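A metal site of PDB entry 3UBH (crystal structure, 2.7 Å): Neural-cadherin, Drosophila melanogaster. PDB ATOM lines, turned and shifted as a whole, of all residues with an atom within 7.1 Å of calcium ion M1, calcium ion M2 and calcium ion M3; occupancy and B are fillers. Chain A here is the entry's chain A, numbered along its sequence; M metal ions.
The side-chain carboxylate (OD1) of Asp 319 sits close to the side-chain amide nitrogen (ND2) of Asn 320 (3.2 Å).
The side-chain carboxylate (OD2) of Asp 316 is in hydrogen-bond range of the side-chain amide nitrogen (ND2) of Asn 357.
The side-chain carboxylate of Asp 316 is in hydrogen-bond range of the backbone NH of Ser 354 (3.0 Å).
The side-chain amide nitrogen (ND2) of Asn 320 sits close to the side-chain carboxylate (OE1) of Glu 283 (3.3 Å).
The side-chain carboxylate (OE1) of Glu 230 sits close to the backbone NH (N) of Phe 282 (2.8 Å).
The backbone NH of Glu 230 is in hydrogen-bond range of the backbone carbonyl oxygen of Thr 315 (3.1 Å).
The backbone NH of Asp 400 lies within hydrogen-bond range of the backbone carbonyl oxygen of Lys 406 (3.2 Å).
N of Gly 402 lies within hydrogen-bond range of OD1 of Asp 400 (2.7 Å).
Four residues have an atom within 4 Å of calcium ion M1: Glu 230, Asp 281, Glu 283 and Asp 319.
The nearest printed residue that does not touch calcium ion M1 is Phe 282 (4.3 Å).
Of the 28 residues printed, 6 come within 4 Å of calcium ion M2.
The nearest printed residue that does not touch calcium ion M2 is Asn 320 (4.3 Å).
The nearest printed residue that does not touch calcium ion M3 is Ala 358 (4.5 Å).
Calcium ion M1 is bound by OD2 of Asp 281 (2.1 Å), OD2 of Asp 319 (2.2 Å), OE1 of Glu 283 (2.5 Å) and OE1 of Glu 230 (2.6 Å).
Calcium ion M1 has four donor atoms within binding distance.
Calcium ion M2 is bound by OD1 of Asp 316 (2.2 Å), O of Val 317 (2.4 Å), OE2 of Glu 230 (2.4 Å), OD1 of Asp 353 (2.5 Å), OE1 of Glu 283 (2.5 Å), OD1 of Asp 319 (2.5 Å) and OE2 of Glu 283 (2.6 Å).
Calcium ion M2 has seven donor atoms within binding distance.
Calcium ion M3 is bound by the backbone carbonyl oxygen (O) of Asn 357, the side-chain amide oxygen (OD1) of Asn 318, the backbone carbonyl oxygen (O) of Asn 320, the side-chain carboxylate (OD2) of Asp 353, the side-chain carboxylate (OD2) of Asp 351, the side-chain carboxylate (OD1) of Asp 351 and the side-chain carboxylate (OD2) of Asp 400.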
ATOM      1  N   GLU A 230      12.940 -18.297   6.874  1.00  0.00           N
ATOM      2  CA  GLU A 230      12.286 -17.009   7.146  1.00  0.00           C
ATOM      3  C   GLU A 230      10.876 -17.106   7.734  1.00  0.00           C
ATOM      4  O   GLU A 230      10.367 -16.123   8.289  1.00  0.00           O
ATOM      5  CB  GLU A 230      12.253 -16.147   5.869  1.00  0.00           C
ATOM      6  CG  GLU A 230      11.251 -16.598   4.796  1.00  0.00           C
ATOM      7  CD  GLU A 230      10.950 -15.541   3.741  1.00  0.00           C
ATOM      8  OE1 GLU A 230      10.953 -14.338   4.070  1.00  0.00           O
ATOM      9  OE2 GLU A 230      10.705 -15.913   2.573  1.00  0.00           O
ATOM     10  N   ASN A 231      10.249 -18.262   7.611  1.00  0.00           N
ATOM     11  CA  ASN A 231       8.861 -18.398   8.012  1.00  0.00           C
ATOM     12  C   ASN A 231       8.693 -19.129   9.333  1.00  0.00           C
ATOM     13  O   ASN A 231       7.575 -19.519   9.696  1.00  0.00           O
ATOM     14  CB  ASN A 231       8.067 -19.130   6.923  1.00  0.00           C
ATOM     15  CG  ASN A 231       8.463 -20.594   6.783  1.00  0.00           C
ATOM     16  OD1 ASN A 231       9.545 -21.024   7.223  1.00  0.00           O
ATOM     17  ND2 ASN A 231       7.594 -21.371   6.150  1.00  0.00           N
ATOM     18  N   LEU A 280      10.538 -13.042  11.046  1.00  0.00           N
ATOM     19  CA  LEU A 280      11.532 -12.724  10.029  1.00  0.00           C
ATOM     20  C   LEU A 280      10.951 -12.421   8.629  1.00  0.00           C
ATOM     21  O   LEU A 280       9.788 -12.714   8.347  1.00  0.00           O
ATOM     22  CB  LEU A 280      12.560 -13.841   9.925  1.00  0.00           C
ATOM     23  CG  LEU A 280      13.296 -14.248  11.201  1.00  0.00           C
ATOM     24  CD1 LEU A 280      13.563 -15.738  11.166  1.00  0.00           C
ATOM     25  CD2 LEU A 280      14.582 -13.452  11.348  1.00  0.00           C
ATOM     26  N   ASP A 281      11.773 -11.824   7.760  1.00  0.00           N
ATOM     27  CA  ASP A 281      11.401 -11.541   6.370  1.00  0.00           C
ATOM     28  C   ASP A 281      12.639 -11.422   5.455  1.00  0.00           C
ATOM     29  O   ASP A 281      13.322 -10.392   5.457  1.00  0.00           O
ATOM     30  CB  ASP A 281      10.515 -10.293   6.279  1.00  0.00           C
ATOM     31  CG  ASP A 281       9.825 -10.160   4.927  1.00  0.00           C
ATOM     32  OD1 ASP A 281       9.396  -9.036   4.607  1.00  0.00           O
ATOM     33  OD2 ASP A 281       9.701 -11.160   4.199  1.00  0.00           O
ATOM     34  N   PHE A 282      12.902 -12.475   4.696  1.00  0.00           N
ATOM     35  CA  PHE A 282      13.987 -12.525   3.713  1.00  0.00           C
ATOM     36  C   PHE A 282      13.862 -11.407   2.702  1.00  0.00           C
ATOM     37  O   PHE A 282      14.858 -10.976   2.121  1.00  0.00           O
ATOM     38  CB  PHE A 282      13.947 -13.869   2.991  1.00  0.00           C
ATOM     39  CG  PHE A 282      15.137 -14.157   2.121  1.00  0.00           C
ATOM     40  CD1 PHE A 282      16.279 -14.763   2.653  1.00  0.00           C
ATOM     41  CD2 PHE A 282      15.103 -13.874   0.761  1.00  0.00           C
ATOM     42  CE1 PHE A 282      17.371 -15.059   1.847  1.00  0.00           C
ATOM     43  CE2 PHE A 282      16.187 -14.151  -0.058  1.00  0.00           C
ATOM     44  CZ  PHE A 282      17.327 -14.741   0.481  1.00  0.00           C
ATOM     45  N   GLU A 283      12.634 -10.935   2.488  1.00  0.00           N
ATOM     46  CA  GLU A 283      12.344  -9.854   1.554  1.00  0.00           C
ATOM     47  C   GLU A 283      12.543  -8.457   2.152  1.00  0.00           C
ATOM     48  O   GLU A 283      12.487  -7.450   1.446  1.00  0.00           O
ATOM     49  CB  GLU A 283      10.913  -9.992   0.992  1.00  0.00           C
ATOM     50  CG  GLU A 283      10.778 -10.989  -0.145  1.00  0.00           C
ATOM     51  CD  GLU A 283      10.954 -12.443   0.292  1.00  0.00           C
ATOM     52  OE1 GLU A 283      10.154 -12.924   1.131  1.00  0.00           O
ATOM     53  OE2 GLU A 283      11.903 -13.094  -0.200  1.00  0.00           O
ATOM     54  N   ASP A 284      12.782  -8.387   3.463  1.00  0.00           N
ATOM     55  CA  ASP A 284      12.983  -7.100   4.123  1.00  0.00           C
ATOM     56  C   ASP A 284      14.459  -6.715   4.119  1.00  0.00           C
ATOM     57  O   ASP A 284      15.266  -7.273   4.874  1.00  0.00           O
ATOM     58  CB  ASP A 284      12.435  -7.136   5.550  1.00  0.00           C
ATOM     59  CG  ASP A 284      12.286  -5.758   6.148  1.00  0.00           C
ATOM     60  OD1 ASP A 284      13.223  -4.943   6.029  1.00  0.00           O
ATOM     61  OD2 ASP A 284      11.230  -5.488   6.757  1.00  0.00           O
ATOM     62  N   THR A 315      16.879 -18.296   5.275  1.00  0.00           N
ATOM     63  CA  THR A 315      16.626 -18.731   3.895  1.00  0.00           C
ATOM     64  C   THR A 315      15.281 -18.266   3.351  1.00  0.00           C
ATOM     65  O   THR A 315      14.319 -18.066   4.086  1.00  0.00           O
ATOM     66  CB  THR A 315      16.715 -20.266   3.743  1.00  0.00           C
ATOM     67  OG1 THR A 315      16.094 -20.886   4.883  1.00  0.00           O
ATOM     68  CG2 THR A 315      18.171 -20.718   3.647  1.00  0.00           C
ATOM     69  N   ASP A 316      15.244 -18.089   2.034  1.00  0.00           N
ATOM     70  CA  ASP A 316      14.055 -17.664   1.304  1.00  0.00           C
ATOM     71  C   ASP A 316      13.026 -18.810   1.263  1.00  0.00           C
ATOM     72  O   ASP A 316      13.360 -19.951   0.946  1.00  0.00           O
ATOM     73  CB  ASP A 316      14.462 -17.223  -0.112  1.00  0.00           C
ATOM     74  CG  ASP A 316      13.269 -16.872  -1.020  1.00  0.00           C
ATOM     75  OD1 ASP A 316      12.275 -16.282  -0.548  1.00  0.00           O
ATOM     76  OD2 ASP A 316      13.350 -17.176  -2.227  1.00  0.00           O
ATOM     77  N   VAL A 317      11.778 -18.496   1.603  1.00  0.00           N
ATOM     78  CA  VAL A 317      10.665 -19.386   1.290  1.00  0.00           C
ATOM     79  C   VAL A 317       9.773 -18.688   0.285  1.00  0.00           C
ATOM     80  O   VAL A 317       9.757 -17.447   0.199  1.00  0.00           O
ATOM     81  CB  VAL A 317       9.852 -19.849   2.542  1.00  0.00           C
ATOM     82  CG1 VAL A 317      10.801 -20.315   3.659  1.00  0.00           C
ATOM     83  CG2 VAL A 317       8.883 -18.762   3.031  1.00  0.00           C
ATOM     84  N   ASN A 318       9.043 -19.471  -0.493  1.00  0.00           N
ATOM     85  CA  ASN A 318       8.164 -18.932  -1.514  1.00  0.00           C
ATOM     86  C   ASN A 318       6.899 -18.365  -0.881  1.00  0.00           C
ATOM     87  O   ASN A 318       5.816 -18.929  -1.041  1.00  0.00           O
ATOM     88  CB  ASN A 318       7.840 -20.000  -2.566  1.00  0.00           C
ATOM     89  CG  ASN A 318       7.094 -19.440  -3.758  1.00  0.00           C
ATOM     90  OD1 ASN A 318       7.458 -18.398  -4.311  1.00  0.00           O
ATOM     91  ND2 ASN A 318       6.029 -20.137  -4.168  1.00  0.00           N
ATOM     92  N   ASP A 319       7.043 -17.270  -0.154  1.00  0.00           N
ATOM     93  CA  ASP A 319       5.885 -16.621   0.490  1.00  0.00           C
ATOM     94  C   ASP A 319       5.246 -15.529  -0.372  1.00  0.00           C
ATOM     95  O   ASP A 319       4.279 -14.893   0.043  1.00  0.00           O
ATOM     96  CB  ASP A 319       6.206 -16.119   1.925  1.00  0.00           C
ATOM     97  CG  ASP A 319       7.473 -15.268   1.997  1.00  0.00           C
ATOM     98  OD1 ASP A 319       8.133 -15.033   0.972  1.00  0.00           O
ATOM     99  OD2 ASP A 319       7.834 -14.839   3.124  1.00  0.00           O
ATOM    100  N   ASN A 320       5.770 -15.310  -1.571  1.00  0.00           N
ATOM    101  CA  ASN A 320       5.217 -14.272  -2.441  1.00  0.00           C
ATOM    102  C   ASN A 320       4.676 -14.779  -3.763  1.00  0.00           C
ATOM    103  O   ASN A 320       5.305 -15.601  -4.435  1.00  0.00           O
ATOM    104  CB  ASN A 320       6.225 -13.152  -2.641  1.00  0.00           C
ATOM    105  CG  ASN A 320       6.315 -12.232  -1.453  1.00  0.00           C
ATOM    106  OD1 ASN A 320       5.431 -11.398  -1.228  1.00  0.00           O
ATOM    107  ND2 ASN A 320       7.375 -12.383  -0.659  1.00  0.00           N
ATOM    108  N   ALA A 321       3.502 -14.290  -4.138  1.00  0.00           N
ATOM    109  CA  ALA A 321       2.932 -14.589  -5.451  1.00  0.00           C
ATOM    110  C   ALA A 321       3.301 -13.521  -6.481  1.00  0.00           C
ATOM    111  O   ALA A 321       3.447 -12.336  -6.137  1.00  0.00           O
ATOM    112  CB  ALA A 321       1.419 -14.747  -5.339  1.00  0.00           C
ATOM    113  N   PRO A 322       3.487 -13.924  -7.759  1.00  0.00           N
ATOM    114  CA  PRO A 322       3.753 -12.920  -8.807  1.00  0.00           C
ATOM    115  C   PRO A 322       2.626 -11.878  -8.854  1.00  0.00           C
ATOM    116  O   PRO A 322       1.458 -12.266  -8.795  1.00  0.00           O
ATOM    117  CB  PRO A 322       3.751 -13.754 -10.099  1.00  0.00           C
ATOM    118  CG  PRO A 322       4.103 -15.143  -9.662  1.00  0.00           C
ATOM    119  CD  PRO A 322       3.481 -15.298  -8.307  1.00  0.00           C
ATOM    120  N   ASP A 351       7.756 -10.672  -8.833  1.00  0.00           N
ATOM    121  CA  ASP A 351       7.722 -11.576  -7.684  1.00  0.00           C
ATOM    122  C   ASP A 351       8.848 -11.211  -6.716  1.00  0.00           C
ATOM    123  O   ASP A 351      10.015 -11.168  -7.112  1.00  0.00           O
ATOM    124  CB  ASP A 351       7.870 -13.029  -8.161  1.00  0.00           C
ATOM    125  CG  ASP A 351       7.530 -14.065  -7.085  1.00  0.00           C
ATOM    126  OD1 ASP A 351       7.890 -13.880  -5.889  1.00  0.00           O
ATOM    127  OD2 ASP A 351       6.910 -15.098  -7.424  1.00  0.00           O
ATOM    128  N   SER A 352       8.482 -10.962  -5.466  1.00  0.00           N
ATOM    129  CA  SER A 352       9.413 -10.537  -4.402  1.00  0.00           C
ATOM    130  C   SER A 352      10.501 -11.547  -4.013  1.00  0.00           C
ATOM    131  O   SER A 352      11.564 -11.148  -3.531  1.00  0.00           O
ATOM    132  CB  SER A 352       8.636 -10.209  -3.131  1.00  0.00           C
ATOM    133  OG  SER A 352       7.769  -9.119  -3.341  1.00  0.00           O
ATOM    134  N   ASP A 353      10.223 -12.837  -4.174  1.00  0.00           N
ATOM    135  CA  ASP A 353      11.112 -13.902  -3.722  1.00  0.00           C
ATOM    136  C   ASP A 353      12.400 -13.953  -4.543  1.00  0.00           C
ATOM    137  O   ASP A 353      12.651 -13.068  -5.373  1.00  0.00           O
ATOM    138  CB  ASP A 353      10.392 -15.264  -3.761  1.00  0.00           C
ATOM    139  CG  ASP A 353       9.118 -15.267  -2.920  1.00  0.00           C
ATOM    140  OD1 ASP A 353       9.159 -14.817  -1.758  1.00  0.00           O
ATOM    141  OD2 ASP A 353       8.074 -15.744  -3.411  1.00  0.00           O
ATOM    142  N   SER A 354      13.232 -14.963  -4.307  1.00  0.00           N
ATOM    143  CA  SER A 354      14.515 -15.076  -5.008  1.00  0.00           C
ATOM    144  C   SER A 354      14.647 -16.378  -5.788  1.00  0.00           C
ATOM    145  O   SER A 354      13.789 -17.253  -5.696  1.00  0.00           O
ATOM    146  CB  SER A 354      15.644 -14.887  -4.025  1.00  0.00           C
ATOM    147  OG  SER A 354      15.421 -13.696  -3.310  1.00  0.00           O
ATOM    148  N   SER A 356      14.368 -19.381  -8.121  1.00  0.00           N
ATOM    149  CA  SER A 356      13.230 -19.924  -8.845  1.00  0.00           C
ATOM    150  C   SER A 356      11.875 -19.675  -8.175  1.00  0.00           C
ATOM    151  O   SER A 356      10.819 -19.837  -8.817  1.00  0.00           O
ATOM    152  CB  SER A 356      13.422 -21.417  -9.139  1.00  0.00           C
ATOM    153  OG  SER A 356      13.488 -22.154  -7.944  1.00  0.00           O
ATOM    154  N   ASN A 357      11.887 -19.275  -6.910  1.00  0.00           N
ATOM    155  CA  ASN A 357      10.651 -18.803  -6.262  1.00  0.00           C
ATOM    156  C   ASN A 357      10.203 -17.483  -6.886  1.00  0.00           C
ATOM    157  O   ASN A 357       9.090 -17.023  -6.630  1.00  0.00           O
ATOM    158  CB  ASN A 357      10.831 -18.631  -4.755  1.00  0.00           C
ATOM    159  CG  ASN A 357      11.063 -19.929  -4.005  1.00  0.00           C
ATOM    160  OD1 ASN A 357      10.550 -20.993  -4.357  1.00  0.00           O
ATOM    161  ND2 ASN A 357      11.821 -19.839  -2.933  1.00  0.00           N
ATOM    162  N   ALA A 358      11.065 -16.885  -7.694  1.00  0.00           N
ATOM    163  CA  ALA A 358      10.765 -15.659  -8.452  1.00  0.00           C
ATOM    164  C   ALA A 358      10.777 -15.846  -9.977  1.00  0.00           C
ATOM    165  O   ALA A 358      10.580 -14.893 -10.733  1.00  0.00           O
ATOM    166  CB  ALA A 358      11.729 -14.556  -8.049  1.00  0.00           C
ATOM    167  N   GLU A 359      11.022 -17.073 -10.434  1.00  0.00           N
ATOM    168  CA  GLU A 359      11.025 -17.394 -11.851  1.00  0.00           C
ATOM    169  C   GLU A 359       9.579 -17.462 -12.338  1.00  0.00           C
ATOM    170  O   GLU A 359       8.751 -18.134 -11.735  1.00  0.00           O
ATOM    171  CB  GLU A 359      11.709 -18.750 -12.070  1.00  0.00           C
ATOM    172  CG  GLU A 359      12.275 -18.968 -13.466  1.00  0.00           C
ATOM    173  CD  GLU A 359      13.714 -18.510 -13.599  1.00  0.00           C
ATOM    174  OE1 GLU A 359      14.077 -18.052 -14.711  1.00  0.00           O
ATOM    175  OE2 GLU A 359      14.482 -18.596 -12.615  1.00  0.00           O
ATOM    176  N   ASP A 400       4.892 -18.815 -10.613  1.00  0.00           N
ATOM    177  CA  ASP A 400       6.297 -18.975 -10.268  1.00  0.00           C
ATOM    178  C   ASP A 400       6.728 -20.434 -10.289  1.00  0.00           C
ATOM    179  O   ASP A 400       5.906 -21.334 -10.472  1.00  0.00           O
ATOM    180  CB  ASP A 400       6.671 -18.271  -8.934  1.00  0.00           C
ATOM    181  CG  ASP A 400       6.096 -18.969  -7.701  1.00  0.00           C
ATOM    182  OD1 ASP A 400       6.065 -20.220  -7.649  1.00  0.00           O
ATOM    183  OD2 ASP A 400       5.693 -18.261  -6.766  1.00  0.00           O
ATOM    184  N   LYS A 401       8.026 -20.665 -10.093  1.00  0.00           N
ATOM    185  CA  LYS A 401       8.567 -22.031 -10.074  1.00  0.00           C
ATOM    186  C   LYS A 401       8.891 -22.512  -8.654  1.00  0.00           C
ATOM    187  O   LYS A 401       9.794 -23.321  -8.448  1.00  0.00           O
ATOM    188  CB  LYS A 401       9.788 -22.147 -10.994  1.00  0.00           C
ATOM    189  CG  LYS A 401       9.504 -21.864 -12.475  1.00  0.00           C
ATOM    190  CD  LYS A 401      10.591 -22.453 -13.387  1.00  0.00           C
ATOM    191  CE  LYS A 401      10.532 -21.890 -14.803  1.00  0.00           C
ATOM    192  NZ  LYS A 401       9.202 -22.099 -15.454  1.00  0.00           N
ATOM    193  N   GLY A 402       8.123 -22.006  -7.682  1.00  0.00           N
ATOM    194  CA  GLY A 402       8.281 -22.416  -6.281  1.00  0.00           C
ATOM    195  C   GLY A 402       7.658 -23.766  -5.995  1.00  0.00           C
ATOM    196  O   GLY A 402       6.997 -24.352  -6.844  1.00  0.00           O
ATOM    197  N   PRO A 405       4.049 -23.952  -6.284  1.00  0.00           N
ATOM    198  CA  PRO A 405       4.039 -22.683  -7.005  1.00  0.00           C
ATOM    199  C   PRO A 405       2.852 -21.788  -6.663  1.00  0.00           C
ATOM    200  O   PRO A 405       1.725 -22.263  -6.563  1.00  0.00           O
ATOM    201  CB  PRO A 405       3.973 -23.120  -8.484  1.00  0.00           C
ATOM    202  CG  PRO A 405       3.285 -24.423  -8.463  1.00  0.00           C
ATOM    203  CD  PRO A 405       3.665 -25.085  -7.160  1.00  0.00           C
ATOM    204  N   LYS A 406       3.125 -20.492  -6.491  1.00  0.00           N
ATOM    205  CA  LYS A 406       2.086 -19.485  -6.252  1.00  0.00           C
ATOM    206  C   LYS A 406       1.740 -18.769  -7.562  1.00  0.00           C
ATOM    207  O   LYS A 406       2.584 -18.663  -8.447  1.00  0.00           O
ATOM    208  CB  LYS A 406       2.557 -18.467  -5.201  1.00  0.00           C
ATOM    209  CG  LYS A 406       2.768 -19.057  -3.806  1.00  0.00           C
ATOM    210  CD  LYS A 406       2.228 -18.116  -2.724  1.00  0.00           C
ATOM    211  CE  LYS A 406       2.661 -18.518  -1.326  1.00  0.00           C
ATOM    212  NZ  LYS A 406       2.225 -19.890  -0.942  1.00  0.00           N
HETATM  213 CA    CA M   1       8.900 -12.950   3.343  1.00  0.00          CA
HETATM  214 CA    CA M   2      10.519 -15.222   0.246  1.00  0.00          CA
HETATM  215 CA    CA M   3       7.210 -16.423  -5.490  1.00  0.00          CA
